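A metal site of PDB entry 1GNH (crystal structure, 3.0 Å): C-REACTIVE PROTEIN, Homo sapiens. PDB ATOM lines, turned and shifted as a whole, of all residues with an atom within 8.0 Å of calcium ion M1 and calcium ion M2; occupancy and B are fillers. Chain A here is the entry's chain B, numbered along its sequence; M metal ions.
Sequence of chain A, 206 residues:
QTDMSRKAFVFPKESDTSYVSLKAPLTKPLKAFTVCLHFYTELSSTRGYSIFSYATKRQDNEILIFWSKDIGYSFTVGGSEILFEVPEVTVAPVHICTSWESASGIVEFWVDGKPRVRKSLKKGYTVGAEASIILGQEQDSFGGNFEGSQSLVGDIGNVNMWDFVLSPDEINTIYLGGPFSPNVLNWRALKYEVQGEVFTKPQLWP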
ATOM      1  N   SER A  50       6.541 -14.727 -27.128  1.00  0.00           N
ATOM      2  CA  SER A  50       7.358 -15.169 -25.992  1.00  0.00           C
ATOM      3  C   SER A  50       6.541 -15.267 -24.706  1.00  0.00           C
ATOM      4  O   SER A  50       5.846 -14.314 -24.313  1.00  0.00           O
ATOM      5  CB  SER A  50       8.545 -14.205 -25.788  1.00  0.00           C
ATOM      6  OG  SER A  50       9.293 -14.569 -24.641  1.00  0.00           O
ATOM      7  N   SER A  53      11.049 -15.527 -20.716  1.00  0.00           N
ATOM      8  CA  SER A  53      12.414 -15.276 -21.213  1.00  0.00           C
ATOM      9  C   SER A  53      13.443 -15.055 -20.095  1.00  0.00           C
ATOM     10  O   SER A  53      13.465 -14.001 -19.432  1.00  0.00           O
ATOM     11  CB  SER A  53      12.426 -14.062 -22.171  1.00  0.00           C
ATOM     12  OG  SER A  53      13.653 -13.941 -22.865  1.00  0.00           O
ATOM     13  N   GLN A  59      24.484 -15.589 -22.506  1.00  0.00           N
ATOM     14  CA  GLN A  59      23.480 -16.261 -23.334  1.00  0.00           C
ATOM     15  C   GLN A  59      22.125 -15.581 -23.165  1.00  0.00           C
ATOM     16  O   GLN A  59      21.530 -15.648 -22.096  1.00  0.00           O
ATOM     17  CB  GLN A  59      23.436 -17.752 -22.937  1.00  0.00           C
ATOM     18  CG  GLN A  59      22.301 -18.562 -23.547  1.00  0.00           C
ATOM     19  CD  GLN A  59      22.322 -18.577 -25.058  1.00  0.00           C
ATOM     20  OE1 GLN A  59      21.804 -17.669 -25.721  1.00  0.00           O
ATOM     21  NE2 GLN A  59      22.903 -19.611 -25.620  1.00  0.00           N
ATOM     22  N   ASP A  60      21.644 -14.943 -24.226  1.00  0.00           N
ATOM     23  CA  ASP A  60      20.356 -14.242 -24.187  1.00  0.00           C
ATOM     24  C   ASP A  60      19.150 -15.174 -24.032  1.00  0.00           C
ATOM     25  O   ASP A  60      18.110 -14.765 -23.523  1.00  0.00           O
ATOM     26  CB  ASP A  60      20.195 -13.337 -25.419  1.00  0.00           C
ATOM     27  CG  ASP A  60      20.217 -14.110 -26.740  1.00  0.00           C
ATOM     28  OD1 ASP A  60      21.156 -14.908 -26.989  1.00  0.00           O
ATOM     29  OD2 ASP A  60      19.279 -13.914 -27.544  1.00  0.00           O
ATOM     30  N   ASN A  61      19.289 -16.412 -24.489  1.00  0.00           N
ATOM     31  CA  ASN A  61      18.183 -17.369 -24.387  1.00  0.00           C
ATOM     32  C   ASN A  61      18.615 -18.528 -23.511  1.00  0.00           C
ATOM     33  O   ASN A  61      18.724 -19.670 -23.997  1.00  0.00           O
ATOM     34  CB  ASN A  61      17.781 -17.872 -25.776  1.00  0.00           C
ATOM     35  CG  ASN A  61      17.170 -16.771 -26.645  1.00  0.00           C
ATOM     36  OD1 ASN A  61      17.205 -16.860 -27.888  1.00  0.00           O
ATOM     37  ND2 ASN A  61      16.593 -15.742 -25.997  1.00  0.00           N
ATOM     38  N   LEU A  64      14.003 -20.334 -22.308  1.00  0.00           N
ATOM     39  CA  LEU A  64      12.917 -19.608 -22.964  1.00  0.00           C
ATOM     40  C   LEU A  64      11.761 -20.517 -23.411  1.00  0.00           C
ATOM     41  O   LEU A  64      11.968 -21.571 -24.008  1.00  0.00           O
ATOM     42  CB  LEU A  64      13.479 -18.840 -24.172  1.00  0.00           C
ATOM     43  CG  LEU A  64      12.520 -18.207 -25.200  1.00  0.00           C
ATOM     44  CD1 LEU A  64      12.603 -16.688 -25.172  1.00  0.00           C
ATOM     45  CD2 LEU A  64      12.861 -18.725 -26.561  1.00  0.00           C
ATOM     46  N   PHE A  66       8.400 -20.503 -25.661  1.00  0.00           N
ATOM     47  CA  PHE A  66       7.846 -19.740 -26.768  1.00  0.00           C
ATOM     48  C   PHE A  66       6.815 -20.547 -27.535  1.00  0.00           C
ATOM     49  O   PHE A  66       6.904 -21.777 -27.609  1.00  0.00           O
ATOM     50  CB  PHE A  66       9.010 -19.435 -27.702  1.00  0.00           C
ATOM     51  CG  PHE A  66       8.713 -18.439 -28.782  1.00  0.00           C
ATOM     52  CD1 PHE A  66       8.239 -18.852 -30.028  1.00  0.00           C
ATOM     53  CD2 PHE A  66       8.977 -17.080 -28.589  1.00  0.00           C
ATOM     54  CE1 PHE A  66       8.017 -17.936 -31.054  1.00  0.00           C
ATOM     55  CE2 PHE A  66       8.770 -16.152 -29.602  1.00  0.00           C
ATOM     56  CZ  PHE A  66       8.289 -16.584 -30.838  1.00  0.00           C
ATOM     57  N   THR A  76      13.372 -23.888 -25.073  1.00  0.00           N
ATOM     58  CA  THR A  76      14.804 -23.777 -25.322  1.00  0.00           C
ATOM     59  C   THR A  76      15.616 -23.424 -24.059  1.00  0.00           C
ATOM     60  O   THR A  76      15.274 -22.498 -23.303  1.00  0.00           O
ATOM     61  CB  THR A  76      15.099 -22.798 -26.532  1.00  0.00           C
ATOM     62  OG1 THR A  76      16.253 -21.987 -26.257  1.00  0.00           O
ATOM     63  CG2 THR A  76      13.897 -21.893 -26.827  1.00  0.00           C
ATOM     64  N   GLN A 137       7.908  -9.974 -23.324  1.00  0.00           N
ATOM     65  CA  GLN A 137       8.789  -9.562 -24.417  1.00  0.00           C
ATOM     66  C   GLN A 137       9.843 -10.618 -24.665  1.00  0.00           C
ATOM     67  O   GLN A 137      10.176 -11.409 -23.769  1.00  0.00           O
ATOM     68  CB  GLN A 137       9.491  -8.233 -24.116  1.00  0.00           C
ATOM     69  CG  GLN A 137       8.659  -7.005 -24.375  1.00  0.00           C
ATOM     70  CD  GLN A 137       8.052  -6.985 -25.766  1.00  0.00           C
ATOM     71  OE1 GLN A 137       7.041  -6.318 -26.000  1.00  0.00           O
ATOM     72  NE2 GLN A 137       8.672  -7.708 -26.713  1.00  0.00           N
ATOM     73  N   GLU A 138      10.414 -10.612 -25.861  1.00  0.00           N
ATOM     74  CA  GLU A 138      11.448 -11.582 -26.193  1.00  0.00           C
ATOM     75  C   GLU A 138      12.831 -10.965 -26.105  1.00  0.00           C
ATOM     76  O   GLU A 138      13.180 -10.107 -26.905  1.00  0.00           O
ATOM     77  CB  GLU A 138      11.210 -12.134 -27.596  1.00  0.00           C
ATOM     78  CG  GLU A 138      11.767 -13.537 -27.822  1.00  0.00           C
ATOM     79  CD  GLU A 138      13.271 -13.584 -27.834  1.00  0.00           C
ATOM     80  OE1 GLU A 138      13.825 -13.393 -28.927  1.00  0.00           O
ATOM     81  OE2 GLU A 138      13.881 -13.838 -26.775  1.00  0.00           O
ATOM     82  N   GLN A 139      13.616 -11.401 -25.126  1.00  0.00           N
ATOM     83  CA  GLN A 139      14.970 -10.890 -24.945  1.00  0.00           C
ATOM     84  C   GLN A 139      15.968 -11.411 -25.952  1.00  0.00           C
ATOM     85  O   GLN A 139      16.060 -12.628 -26.206  1.00  0.00           O
ATOM     86  CB  GLN A 139      15.509 -11.209 -23.549  1.00  0.00           C
ATOM     87  CG  GLN A 139      15.328 -10.110 -22.559  1.00  0.00           C
ATOM     88  CD  GLN A 139      15.386 -10.632 -21.145  1.00  0.00           C
ATOM     89  OE1 GLN A 139      14.374 -11.050 -20.602  1.00  0.00           O
ATOM     90  NE2 GLN A 139      16.591 -10.663 -20.562  1.00  0.00           N
ATOM     91  N   ASP A 140      16.748 -10.484 -26.488  1.00  0.00           N
ATOM     92  CA  ASP A 140      17.792 -10.797 -27.459  1.00  0.00           C
ATOM     93  C   ASP A 140      19.106 -10.175 -27.008  1.00  0.00           C
ATOM     94  O   ASP A 140      20.108 -10.164 -27.745  1.00  0.00           O
ATOM     95  CB  ASP A 140      17.398 -10.332 -28.860  1.00  0.00           C
ATOM     96  CG  ASP A 140      16.341 -11.223 -29.480  1.00  0.00           C
ATOM     97  OD1 ASP A 140      16.425 -12.463 -29.309  1.00  0.00           O
ATOM     98  OD2 ASP A 140      15.410 -10.698 -30.121  1.00  0.00           O
ATOM     99  N   SER A 141      19.081  -9.678 -25.784  1.00  0.00           N
ATOM    100  CA  SER A 141      20.213  -9.063 -25.126  1.00  0.00           C
ATOM    101  C   SER A 141      19.792  -8.957 -23.666  1.00  0.00           C
ATOM    102  O   SER A 141      18.588  -8.881 -23.356  1.00  0.00           O
ATOM    103  CB  SER A 141      20.532  -7.661 -25.709  1.00  0.00           C
ATOM    104  OG  SER A 141      19.722  -6.618 -25.157  1.00  0.00           O
ATOM    105  N   GLY A 144      17.048  -6.454 -22.820  1.00  0.00           N
ATOM    106  CA  GLY A 144      16.621  -5.630 -23.935  1.00  0.00           C
ATOM    107  C   GLY A 144      16.585  -6.299 -25.299  1.00  0.00           C
ATOM    108  O   GLY A 144      16.611  -7.535 -25.408  1.00  0.00           O
ATOM    109  N   ASN A 145      16.532  -5.449 -26.337  1.00  0.00           N
ATOM    110  CA  ASN A 145      16.471  -5.881 -27.741  1.00  0.00           C
ATOM    111  C   ASN A 145      15.171  -6.654 -27.993  1.00  0.00           C
ATOM    112  O   ASN A 145      15.185  -7.818 -28.433  1.00  0.00           O
ATOM    113  CB  ASN A 145      17.711  -6.718 -28.133  1.00  0.00           C
ATOM    114  CG  ASN A 145      18.940  -5.842 -28.473  1.00  0.00           C
ATOM    115  OD1 ASN A 145      19.448  -5.074 -27.633  1.00  0.00           O
ATOM    116  ND2 ASN A 145      19.420  -5.954 -29.704  1.00  0.00           N
ATOM    117  N   PHE A 146      14.056  -5.971 -27.751  1.00  0.00           N
ATOM    118  CA  PHE A 146      12.720  -6.552 -27.902  1.00  0.00           C
ATOM    119  C   PHE A 146      12.135  -6.466 -29.302  1.00  0.00           C
ATOM    120  O   PHE A 146      12.025  -5.369 -29.874  1.00  0.00           O
ATOM    121  CB  PHE A 146      11.748  -5.892 -26.913  1.00  0.00           C
ATOM    122  CG  PHE A 146      12.198  -5.935 -25.484  1.00  0.00           C
ATOM    123  CD1 PHE A 146      12.863  -7.059 -24.984  1.00  0.00           C
ATOM    124  CD2 PHE A 146      11.980  -4.845 -24.650  1.00  0.00           C
ATOM    125  CE1 PHE A 146      13.303  -7.083 -23.657  1.00  0.00           C
ATOM    126  CE2 PHE A 146      12.413  -4.860 -23.332  1.00  0.00           C
ATOM    127  CZ  PHE A 146      13.080  -5.976 -22.825  1.00  0.00           C
ATOM    128  N   GLU A 147      11.780  -7.621 -29.881  1.00  0.00           N
ATOM    129  CA  GLU A 147      11.141  -7.554 -31.172  1.00  0.00           C
ATOM    130  C   GLU A 147       9.650  -7.715 -30.938  1.00  0.00           C
ATOM    131  O   GLU A 147       9.176  -8.653 -30.270  1.00  0.00           O
ATOM    132  CB  GLU A 147      11.743  -8.423 -32.291  1.00  0.00           C
ATOM    133  CG  GLU A 147      11.748  -7.677 -33.678  1.00  0.00           C
ATOM    134  CD  GLU A 147      12.593  -6.354 -33.732  1.00  0.00           C
ATOM    135  OE1 GLU A 147      12.639  -5.560 -32.756  1.00  0.00           O
ATOM    136  OE2 GLU A 147      13.188  -6.099 -34.805  1.00  0.00           O
ATOM    137  N   GLY A 148       8.932  -6.681 -31.391  1.00  0.00           N
ATOM    138  CA  GLY A 148       7.478  -6.585 -31.228  1.00  0.00           C
ATOM    139  C   GLY A 148       6.674  -7.699 -31.858  1.00  0.00           C
ATOM    140  O   GLY A 148       5.521  -7.906 -31.509  1.00  0.00           O
ATOM    141  N   SER A 149       7.295  -8.420 -32.791  1.00  0.00           N
ATOM    142  CA  SER A 149       6.680  -9.547 -33.489  1.00  0.00           C
ATOM    143  C   SER A 149       6.662 -10.789 -32.577  1.00  0.00           C
ATOM    144  O   SER A 149       6.163 -11.865 -32.940  1.00  0.00           O
ATOM    145  CB  SER A 149       7.496  -9.833 -34.773  1.00  0.00           C
ATOM    146  OG  SER A 149       6.892 -10.822 -35.597  1.00  0.00           O
ATOM    147  N   GLN A 150       7.218 -10.643 -31.373  1.00  0.00           N
ATOM    148  CA  GLN A 150       7.291 -11.730 -30.424  1.00  0.00           C
ATOM    149  C   GLN A 150       6.779 -11.281 -29.062  1.00  0.00           C
ATOM    150  O   GLN A 150       7.066 -11.905 -28.047  1.00  0.00           O
ATOM    151  CB  GLN A 150       8.745 -12.196 -30.323  1.00  0.00           C
ATOM    152  CG  GLN A 150       9.377 -12.474 -31.679  1.00  0.00           C
ATOM    153  CD  GLN A 150      10.710 -13.209 -31.578  1.00  0.00           C
ATOM    154  OE1 GLN A 150      11.627 -12.785 -30.866  1.00  0.00           O
ATOM    155  NE2 GLN A 150      10.824 -14.310 -32.311  1.00  0.00           N
ATOM    156  N   SER A 151       6.036 -10.182 -29.046  1.00  0.00           N
ATOM    157  CA  SER A 151       5.500  -9.665 -27.792  1.00  0.00           C
ATOM    158  C   SER A 151       4.247 -10.455 -27.435  1.00  0.00           C
ATOM    159  O   SER A 151       3.635 -11.093 -28.301  1.00  0.00           O
ATOM    160  CB  SER A 151       5.160  -8.173 -27.920  1.00  0.00           C
ATOM    161  OG  SER A 151       4.697  -7.659 -26.673  1.00  0.00           O
HETATM  162 CA    CA M   1      13.695 -11.842 -30.482  1.00  0.00          CA
HETATM  163 CA    CA M   2      15.109 -14.609 -28.553  1.00  0.00          CA
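Residues that only touch calcium ion M2: Gln 139 (3.2 Å).
The backbone carbonyl oxygen (O) of Gln 139 sits at hydrogen-bond distance from the side-chain amide nitrogen (ND2) of Asn 61 (3.2 Å).
The backbone NH of Asn 61 is in hydrogen-bond range of the side-chain amide oxygen of Gln 59, at 3.1 Å.
OE1 of Gln 139 lies close to O of Ser 53 (3.3 Å).
O of Gln 150 is in hydrogen-bond range of N of Ser 50 (3.0 Å).
The side-chain amide nitrogen (ND2) of Asn 61 sits close to the side-chain carboxylate (OE2) of Glu 138 (3.4 Å).
Calcium ion M2 is bound by the side-chain carboxylate (OE1) of Glu 138, the side-chain carboxylate (OE2) of Glu 138 and the side-chain carboxylate (OD1) of Asp 140.
Slightly farther from calcium ion M2 lies the side-chain amide oxygen (OD1) of Asn 61 (3.1 Å).
Calcium ion M1 is bound by the side-chain carboxylate (OD2) of Asp 140 (2.1 Å), the side-chain carboxylate (OE1) of Glu 138 (2.2 Å) and the side-chain amide oxygen (OE1) of Gln 150 (2.3 Å).
Slightly farther from calcium ion M1 lies OD1 of Asp 140 (3.0 Å).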
